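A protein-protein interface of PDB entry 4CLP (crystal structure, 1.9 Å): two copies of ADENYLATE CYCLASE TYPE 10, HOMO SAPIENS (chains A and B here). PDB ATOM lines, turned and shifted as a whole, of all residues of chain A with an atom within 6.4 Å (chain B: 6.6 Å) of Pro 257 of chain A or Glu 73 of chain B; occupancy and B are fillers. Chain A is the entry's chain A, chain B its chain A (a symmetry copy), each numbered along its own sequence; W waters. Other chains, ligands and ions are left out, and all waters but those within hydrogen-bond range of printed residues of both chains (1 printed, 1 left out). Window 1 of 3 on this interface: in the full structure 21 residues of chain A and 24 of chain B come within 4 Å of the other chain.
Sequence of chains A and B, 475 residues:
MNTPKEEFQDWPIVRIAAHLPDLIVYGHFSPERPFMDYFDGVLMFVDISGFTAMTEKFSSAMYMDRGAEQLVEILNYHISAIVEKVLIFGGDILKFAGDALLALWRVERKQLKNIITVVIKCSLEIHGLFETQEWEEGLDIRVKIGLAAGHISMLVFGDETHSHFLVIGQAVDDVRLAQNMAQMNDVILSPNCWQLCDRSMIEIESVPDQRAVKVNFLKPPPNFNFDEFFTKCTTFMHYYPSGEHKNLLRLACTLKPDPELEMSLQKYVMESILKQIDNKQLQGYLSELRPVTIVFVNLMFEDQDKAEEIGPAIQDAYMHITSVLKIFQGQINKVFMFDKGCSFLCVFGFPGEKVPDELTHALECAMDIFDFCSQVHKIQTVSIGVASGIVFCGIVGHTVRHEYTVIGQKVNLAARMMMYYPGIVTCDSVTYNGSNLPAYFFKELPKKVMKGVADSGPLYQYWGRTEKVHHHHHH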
ATOM      1  N   TRP A  11     -16.992  28.774  -1.967  1.00  0.00           N
ATOM      2  CA  TRP A  11     -15.707  28.091  -1.907  1.00  0.00           C
ATOM      3  C   TRP A  11     -15.164  27.795  -3.291  1.00  0.00           C
ATOM      4  O   TRP A  11     -15.969  27.595  -4.231  1.00  0.00           O
ATOM      5  CB  TRP A  11     -15.904  26.784  -1.185  1.00  0.00           C
ATOM      6  CG  TRP A  11     -16.402  26.887   0.204  1.00  0.00           C
ATOM      7  CD1 TRP A  11     -17.636  26.524   0.629  1.00  0.00           C
ATOM      8  CD2 TRP A  11     -15.690  27.326   1.359  1.00  0.00           C
ATOM      9  NE1 TRP A  11     -17.723  26.699   1.967  1.00  0.00           N
ATOM     10  CE2 TRP A  11     -16.543  27.208   2.437  1.00  0.00           C
ATOM     11  CE3 TRP A  11     -14.436  27.815   1.570  1.00  0.00           C
ATOM     12  CZ2 TRP A  11     -16.174  27.579   3.735  1.00  0.00           C
ATOM     13  CZ3 TRP A  11     -14.043  28.167   2.828  1.00  0.00           C
ATOM     14  CH2 TRP A  11     -14.935  28.090   3.913  1.00  0.00           C
ATOM     15  N   PRO A  12     -13.826  27.670  -3.405  1.00  0.00           N
ATOM     16  CA  PRO A  12     -13.237  27.285  -4.639  1.00  0.00           C
ATOM     17  C   PRO A  12     -13.815  26.023  -5.249  1.00  0.00           C
ATOM     18  O   PRO A  12     -14.045  25.997  -6.460  1.00  0.00           O
ATOM     19  CB  PRO A  12     -11.781  27.030  -4.278  1.00  0.00           C
ATOM     20  CG  PRO A  12     -11.529  28.023  -3.204  1.00  0.00           C
ATOM     21  CD  PRO A  12     -12.802  28.036  -2.407  1.00  0.00           C
ATOM     22  N   ILE A  13     -14.113  24.992  -4.460  1.00  0.00           N
ATOM     23  CA  ILE A  13     -14.752  23.770  -5.050  1.00  0.00           C
ATOM     24  C   ILE A  13     -16.099  24.087  -5.754  1.00  0.00           C
ATOM     25  O   ILE A  13     -16.401  23.490  -6.790  1.00  0.00           O
ATOM     26  CB  ILE A  13     -14.888  22.618  -4.049  1.00  0.00           C
ATOM     27  CG1 ILE A  13     -14.942  21.245  -4.708  1.00  0.00           C
ATOM     28  CG2 ILE A  13     -15.993  22.906  -2.995  1.00  0.00           C
ATOM     29  CD1 ILE A  13     -14.895  20.110  -3.646  1.00  0.00           C
ATOM     30  N   VAL A  14     -16.885  25.003  -5.198  1.00  0.00           N
ATOM     31  CA  VAL A  14     -18.174  25.359  -5.816  1.00  0.00           C
ATOM     32  C   VAL A  14     -17.920  26.113  -7.127  1.00  0.00           C
ATOM     33  O   VAL A  14     -18.501  25.859  -8.133  1.00  0.00           O
ATOM     34  CB  VAL A  14     -19.045  26.194  -4.838  1.00  0.00           C
ATOM     35  CG1 VAL A  14     -20.253  26.762  -5.545  1.00  0.00           C
ATOM     36  CG2 VAL A  14     -19.471  25.395  -3.624  1.00  0.00           C
ATOM     37  N   LEU A 255     -21.976  22.165  -2.638  1.00  0.00           N
ATOM     38  CA  LEU A 255     -20.807  21.346  -2.427  1.00  0.00           C
ATOM     39  C   LEU A 255     -19.888  21.941  -1.340  1.00  0.00           C
ATOM     40  O   LEU A 255     -19.702  23.157  -1.266  1.00  0.00           O
ATOM     41  CB  LEU A 255     -19.982  21.264  -3.708  1.00  0.00           C
ATOM     42  CG  LEU A 255     -20.144  20.303  -4.821  1.00  0.00           C
ATOM     43  CD1 LEU A 255     -18.880  20.474  -5.737  1.00  0.00           C
ATOM     44  CD2 LEU A 255     -20.208  18.876  -4.276  1.00  0.00           C
ATOM     45  N   LYS A 256     -19.316  21.082  -0.530  1.00  0.00           N
ATOM     46  CA  LYS A 256     -18.512  21.498   0.613  1.00  0.00           C
ATOM     47  C   LYS A 256     -17.046  21.163   0.282  1.00  0.00           C
ATOM     48  O   LYS A 256     -16.763  20.211  -0.433  1.00  0.00           O
ATOM     49  CB  LYS A 256     -18.927  20.781   1.880  1.00  0.00           C
ATOM     50  CG  LYS A 256     -20.354  21.107   2.344  1.00  0.00           C
ATOM     51  CD  LYS A 256     -20.634  22.595   2.221  1.00  0.00           C
ATOM     52  CE  LYS A 256     -22.095  22.855   2.582  1.00  0.00           C
ATOM     53  NZ  LYS A 256     -22.471  24.238   2.211  1.00  0.00           N
ATOM     54  N   PRO A 257     -16.123  21.958   0.816  1.00  0.00           N
ATOM     55  CA  PRO A 257     -14.730  21.632   0.625  1.00  0.00           C
ATOM     56  C   PRO A 257     -14.399  20.157   0.864  1.00  0.00           C
ATOM     57  O   PRO A 257     -14.833  19.546   1.828  1.00  0.00           O
ATOM     58  CB  PRO A 257     -14.048  22.531   1.660  1.00  0.00           C
ATOM     59  CG  PRO A 257     -14.837  23.752   1.543  1.00  0.00           C
ATOM     60  CD  PRO A 257     -16.246  23.182   1.582  1.00  0.00           C
ATOM     61  N   ASP A 258     -13.517  19.627   0.059  1.00  0.00           N
ATOM     62  CA  ASP A 258     -13.187  18.249   0.102  1.00  0.00           C
ATOM     63  C   ASP A 258     -11.976  18.105  -0.841  1.00  0.00           C
ATOM     64  O   ASP A 258     -12.147  18.081  -2.047  1.00  0.00           O
ATOM     65  CB  ASP A 258     -14.339  17.431  -0.505  1.00  0.00           C
ATOM     66  CG  ASP A 258     -13.992  15.894  -0.589  1.00  0.00           C
ATOM     67  OD1 ASP A 258     -12.806  15.486  -0.606  1.00  0.00           O
ATOM     68  OD2 ASP A 258     -14.964  15.181  -0.608  1.00  0.00           O
ATOM     69  N   PRO A 259     -10.791  18.105  -0.300  1.00  0.00           N
ATOM     70  CA  PRO A 259      -9.587  18.209  -1.153  1.00  0.00           C
ATOM     71  C   PRO A 259      -9.438  17.094  -2.193  1.00  0.00           C
ATOM     72  O   PRO A 259      -8.998  17.343  -3.298  1.00  0.00           O
ATOM     73  CB  PRO A 259      -8.448  18.107  -0.151  1.00  0.00           C
ATOM     74  CG  PRO A 259      -9.012  18.504   1.167  1.00  0.00           C
ATOM     75  CD  PRO A 259     -10.478  18.230   1.134  1.00  0.00           C
ATOM     76  N   GLU A 262     -11.895  17.960  -4.943  1.00  0.00           N
ATOM     77  CA  GLU A 262     -11.404  19.142  -5.677  1.00  0.00           C
ATOM     78  C   GLU A 262     -10.228  18.760  -6.562  1.00  0.00           C
ATOM     79  O   GLU A 262     -10.133  19.237  -7.683  1.00  0.00           O
ATOM     80  CB  GLU A 262     -11.023  20.286  -4.763  1.00  0.00           C
ATOM     81  CG  GLU A 262     -10.649  21.573  -5.511  1.00  0.00           C
ATOM     82  CD  GLU A 262     -10.532  22.799  -4.619  1.00  0.00           C
ATOM     83  OE1 GLU A 262     -11.407  22.897  -3.727  1.00  0.00           O
ATOM     84  OE2 GLU A 262      -9.611  23.661  -4.818  1.00  0.00           O
ATOM     85  N   ARG B  66      -1.803  23.817  -6.452  1.00  0.00           N
ATOM     86  CA  ARG B  66      -2.849  24.562  -5.764  1.00  0.00           C
ATOM     87  C   ARG B  66      -2.908  24.147  -4.336  1.00  0.00           C
ATOM     88  O   ARG B  66      -3.905  24.322  -3.658  1.00  0.00           O
ATOM     89  CB  ARG B  66      -4.233  24.416  -6.478  1.00  0.00           C
ATOM     90  CG  ARG B  66      -4.292  25.251  -7.755  1.00  0.00           C
ATOM     91  CD  ARG B  66      -5.639  25.147  -8.484  1.00  0.00           C
ATOM     92  NE  ARG B  66      -6.654  25.790  -7.663  1.00  0.00           N
ATOM     93  CZ  ARG B  66      -7.528  25.180  -6.873  1.00  0.00           C
ATOM     94  NH1 ARG B  66      -7.632  23.847  -6.804  1.00  0.00           N
ATOM     95  NH2 ARG B  66      -8.348  25.910  -6.189  1.00  0.00           N
ATOM     96  N   ALA B  68      -1.651  25.661  -1.578  1.00  0.00           N
ATOM     97  CA  ALA B  68      -2.050  26.747  -0.677  1.00  0.00           C
ATOM     98  C   ALA B  68      -3.540  27.048  -0.710  1.00  0.00           C
ATOM     99  O   ALA B  68      -4.182  27.270   0.347  1.00  0.00           O
ATOM    100  CB  ALA B  68      -1.270  28.005  -1.012  1.00  0.00           C
ATOM    101  N   GLU B  69      -4.086  27.073  -1.924  1.00  0.00           N
ATOM    102  CA  GLU B  69      -5.527  27.307  -2.103  1.00  0.00           C
ATOM    103  C   GLU B  69      -6.375  26.234  -1.484  1.00  0.00           C
ATOM    104  O   GLU B  69      -7.381  26.521  -0.759  1.00  0.00           O
ATOM    105  CB  GLU B  69      -5.832  27.406  -3.553  1.00  0.00           C
ATOM    106  CG  GLU B  69      -5.183  28.638  -4.178  1.00  0.00           C
ATOM    107  CD  GLU B  69      -3.718  28.528  -4.513  1.00  0.00           C
ATOM    108  OE1 GLU B  69      -3.063  27.467  -4.471  1.00  0.00           O
ATOM    109  OE2 GLU B  69      -3.181  29.575  -4.788  1.00  0.00           O
ATOM    110  N   GLN B  70      -5.972  24.996  -1.701  1.00  0.00           N
ATOM    111  CA  GLN B  70      -6.735  23.839  -1.134  1.00  0.00           C
ATOM    112  C   GLN B  70      -6.605  23.817   0.399  1.00  0.00           C
ATOM    113  O   GLN B  70      -7.577  23.584   1.121  1.00  0.00           O
ATOM    114  CB  GLN B  70      -6.150  22.568  -1.704  1.00  0.00           C
ATOM    115  CG  GLN B  70      -6.609  22.332  -3.137  1.00  0.00           C
ATOM    116  CD  GLN B  70      -7.569  21.187  -3.214  1.00  0.00           C
ATOM    117  OE1 GLN B  70      -8.530  21.046  -2.406  1.00  0.00           O
ATOM    118  NE2 GLN B  70      -7.368  20.386  -4.218  1.00  0.00           N
ATOM    119  N   LEU B  71      -5.418  24.128   0.908  1.00  0.00           N
ATOM    120  CA  LEU B  71      -5.196  24.118   2.347  1.00  0.00           C
ATOM    121  C   LEU B  71      -6.048  25.162   3.029  1.00  0.00           C
ATOM    122  O   LEU B  71      -6.747  24.873   4.005  1.00  0.00           O
ATOM    123  CB  LEU B  71      -3.710  24.292   2.678  1.00  0.00           C
ATOM    124  CG  LEU B  71      -3.314  24.226   4.164  1.00  0.00           C
ATOM    125  CD1 LEU B  71      -3.548  22.824   4.739  1.00  0.00           C
ATOM    126  CD2 LEU B  71      -1.861  24.697   4.353  1.00  0.00           C
ATOM    127  N   VAL B  72      -6.015  26.376   2.558  1.00  0.00           N
ATOM    128  CA  VAL B  72      -6.767  27.417   3.221  1.00  0.00           C
ATOM    129  C   VAL B  72      -8.257  27.199   3.150  1.00  0.00           C
ATOM    130  O   VAL B  72      -8.990  27.498   4.121  1.00  0.00           O
ATOM    131  CB  VAL B  72      -6.338  28.813   2.816  1.00  0.00           C
ATOM    132  CG1 VAL B  72      -6.897  29.253   1.511  1.00  0.00           C
ATOM    133  CG2 VAL B  72      -6.759  29.827   3.905  1.00  0.00           C
ATOM    134  N   GLU B  73      -8.732  26.656   2.030  1.00  0.00           N
ATOM    135  CA  GLU B  73     -10.138  26.315   1.928  1.00  0.00           C
ATOM    136  C   GLU B  73     -10.598  25.277   2.955  1.00  0.00           C
ATOM    137  O   GLU B  73     -11.637  25.437   3.605  1.00  0.00           O
ATOM    138  CB  GLU B  73     -10.395  25.812   0.504  1.00  0.00           C
ATOM    139  CG  GLU B  73     -11.848  25.366   0.224  1.00  0.00           C
ATOM    140  CD  GLU B  73     -11.994  24.892  -1.214  1.00  0.00           C
ATOM    141  OE1 GLU B  73     -10.937  24.547  -1.835  1.00  0.00           O
ATOM    142  OE2 GLU B  73     -13.146  24.779  -1.667  1.00  0.00           O
ATOM    143  N   ILE B  74      -9.911  24.157   3.008  1.00  0.00           N
ATOM    144  CA  ILE B  74     -10.341  23.100   3.947  1.00  0.00           C
ATOM    145  C   ILE B  74     -10.129  23.573   5.366  1.00  0.00           C
ATOM    146  O   ILE B  74     -10.948  23.325   6.208  1.00  0.00           O
ATOM    147  CB  ILE B  74      -9.659  21.751   3.663  1.00  0.00           C
ATOM    148  CG1 ILE B  74     -10.400  20.589   4.307  1.00  0.00           C
ATOM    149  CG2 ILE B  74      -8.198  21.716   4.018  1.00  0.00           C
ATOM    150  CD1 ILE B  74     -11.894  20.501   4.034  1.00  0.00           C
ATOM    151  N   LEU B  75      -9.045  24.268   5.627  1.00  0.00           N
ATOM    152  CA  LEU B  75      -8.871  24.814   7.006  1.00  0.00           C
ATOM    153  C   LEU B  75      -9.970  25.788   7.394  1.00  0.00           C
ATOM    154  O   LEU B  75     -10.532  25.660   8.488  1.00  0.00           O
ATOM    155  CB  LEU B  75      -7.503  25.441   7.134  1.00  0.00           C
ATOM    156  CG  LEU B  75      -7.281  26.054   8.521  1.00  0.00           C
ATOM    157  CD1 LEU B  75      -7.306  24.969   9.592  1.00  0.00           C
ATOM    158  CD2 LEU B  75      -5.977  26.821   8.552  1.00  0.00           C
ATOM    159  N   ASN B  76     -10.238  26.771   6.524  1.00  0.00           N
ATOM    160  CA  ASN B  76     -11.261  27.754   6.837  1.00  0.00           C
ATOM    161  C   ASN B  76     -12.662  27.168   6.956  1.00  0.00           C
ATOM    162  O   ASN B  76     -13.481  27.611   7.792  1.00  0.00           O
ATOM    163  CB  ASN B  76     -11.196  28.912   5.920  1.00  0.00           C
ATOM    164  CG  ASN B  76     -10.075  29.857   6.284  1.00  0.00           C
ATOM    165  OD1 ASN B  76      -9.494  29.732   7.358  1.00  0.00           O
ATOM    166  ND2 ASN B  76      -9.800  30.790   5.451  1.00  0.00           N
ATOM    167  N   TYR B  77     -12.919  26.097   6.234  1.00  0.00           N
ATOM    168  CA  TYR B  77     -14.219  25.434   6.326  1.00  0.00           C
ATOM    169  C   TYR B  77     -14.440  24.924   7.760  1.00  0.00           C
ATOM    170  O   TYR B  77     -15.489  25.128   8.384  1.00  0.00           O
ATOM    171  CB  TYR B  77     -14.310  24.322   5.309  1.00  0.00           C
ATOM    172  CG  TYR B  77     -15.556  23.507   5.374  1.00  0.00           C
ATOM    173  CD1 TYR B  77     -16.801  24.095   5.235  1.00  0.00           C
ATOM    174  CD2 TYR B  77     -15.496  22.160   5.520  1.00  0.00           C
ATOM    175  CE1 TYR B  77     -17.958  23.332   5.288  1.00  0.00           C
ATOM    176  CE2 TYR B  77     -16.669  21.388   5.540  1.00  0.00           C
ATOM    177  CZ  TYR B  77     -17.873  22.007   5.425  1.00  0.00           C
ATOM    178  OH  TYR B  77     -19.012  21.236   5.447  1.00  0.00           O
ATOM    179  N   HIS B  78     -13.424  24.310   8.282  1.00  0.00           N
ATOM    180  CA  HIS B  78     -13.490  23.782   9.649  1.00  0.00           C
ATOM    181  C   HIS B  78     -13.387  24.877  10.693  1.00  0.00           C
ATOM    182  O   HIS B  78     -14.152  24.873  11.627  1.00  0.00           O
ATOM    183  CB  HIS B  78     -12.393  22.726   9.883  1.00  0.00           C
ATOM    184  CG  HIS B  78     -12.606  21.493   9.099  1.00  0.00           C
ATOM    185  ND1 HIS B  78     -13.737  20.712   9.246  1.00  0.00           N
ATOM    186  CD2 HIS B  78     -11.895  20.937   8.096  1.00  0.00           C
ATOM    187  CE1 HIS B  78     -13.688  19.709   8.377  1.00  0.00           C
ATOM    188  NE2 HIS B  78     -12.588  19.834   7.670  1.00  0.00           N
HETATM  189  O   HOH W   1     -12.007  21.507  -1.378  1.00  0.00           O
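Trp 11 of chain A touches Glu 73 of chain B (CB to OE2, 3.4 Å).
Trp 11 of chain A touches Asn 76 of chain B (CH2 to C, 3.9 Å).
Tyr 77 of chain B touches Trp 11 of chain A (CA to CH2, 3.7 Å).
Lys 256 of chain A touches Tyr 77 of chain B (CG to OH, 3.4 Å).
Pro 257 of chain A touches Glu 73 of chain B (CG to CG, 3.6 Å).
Ile 74 of chain B touches Pro 257 of chain A.
CD of Pro 257 of chain A touches CD1 of Tyr 77 of chain B (3.8 Å).
Pro 259 of chain A touches Gln 70 of chain B.
Ile 74 of chain B touches Pro 259 of chain A (CD1 to CD, 3.9 Å).
Gln 70 of chain B touches Glu 262 of chain A (OE1 to CD, 3.5 Å).
Of the 12 printed residues of chain B, 6 touch a printed residue of chain A.
Printed residues of chain B that touch a printed residue of chain A: Arg 66, Gln 70, Glu 73, Ile 74, Asn 76 and Tyr 77.
Hydrophobic or aromatic side chains of chain B within 4 Å of the printed part of chain A: Ile 74 and Tyr 77.
Water W1 lies within hydrogen-bond range of the side-chain carboxylate (OE1) of Glu 262 of chain A, the backbone NH (N) of Asp 258 of chain A and the side-chain carboxylate (OE1) of Glu 73 of chain B.
N of Ile 13 of chain A lies within hydrogen-bond range of OE1 of Glu 262 of chain A, 3.5 Å away.
OE2 of Glu 73 of chain B sits close to N of Pro 12 of chain A, 3.4 Å away.
The backbone NH (N) of Ile 13 of chain A lies within hydrogen-bond range of the side-chain carboxylate (OE2) of Glu 73 of chain B (3.0 Å).
The side-chain carboxylate (OE2) of Glu 262 of chain A is in salt-bridge range of the guanidinium group (NH1) of Arg 66 of chain B (2.8 Å).
OE1 of Glu 262 of chain A sits close to OE1 of Glu 73 of chain B (2.6 Å).
No position is printed for both chains.
Of the 14 pairs that touch across the chains among the printed residues, none has its exchanged pair printed and touching as well.
Of chain B, only Glu 73 (3.6 Å), Ile 74 (3.8 Å) and Tyr 77 (3.8 Å) come within 4 Å of Pro 257 of chain A.
Glu 73 of chain B touches five residues of chain A.
Of the printed residues of chain B, Trp 11 of chain A touches Glu 73, Asn 76 and Tyr 77.
Printed residues of chain B within 4 Å of Pro 12 of chain A: Glu 73.
Printed residues of chain A within 4 Å of Arg 66 of chain B: Glu 262.
Printed residues of chain A within 4 Å of Ile 74 of chain B: Pro 257 (3.8 Å) and Pro 259 (3.9 Å).
Printed residues of chain B within 4 Å of Ile 13 of chain A: Glu 73 (3.0 Å).
The nearest residue of chain A that does not touch Glu 73 of chain B is Val 14 of chain A (5.1 Å).
The nearest printed residue of chain B that does not touch Pro 259 of chain A is Glu 73 of chain B (6.5 Å).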
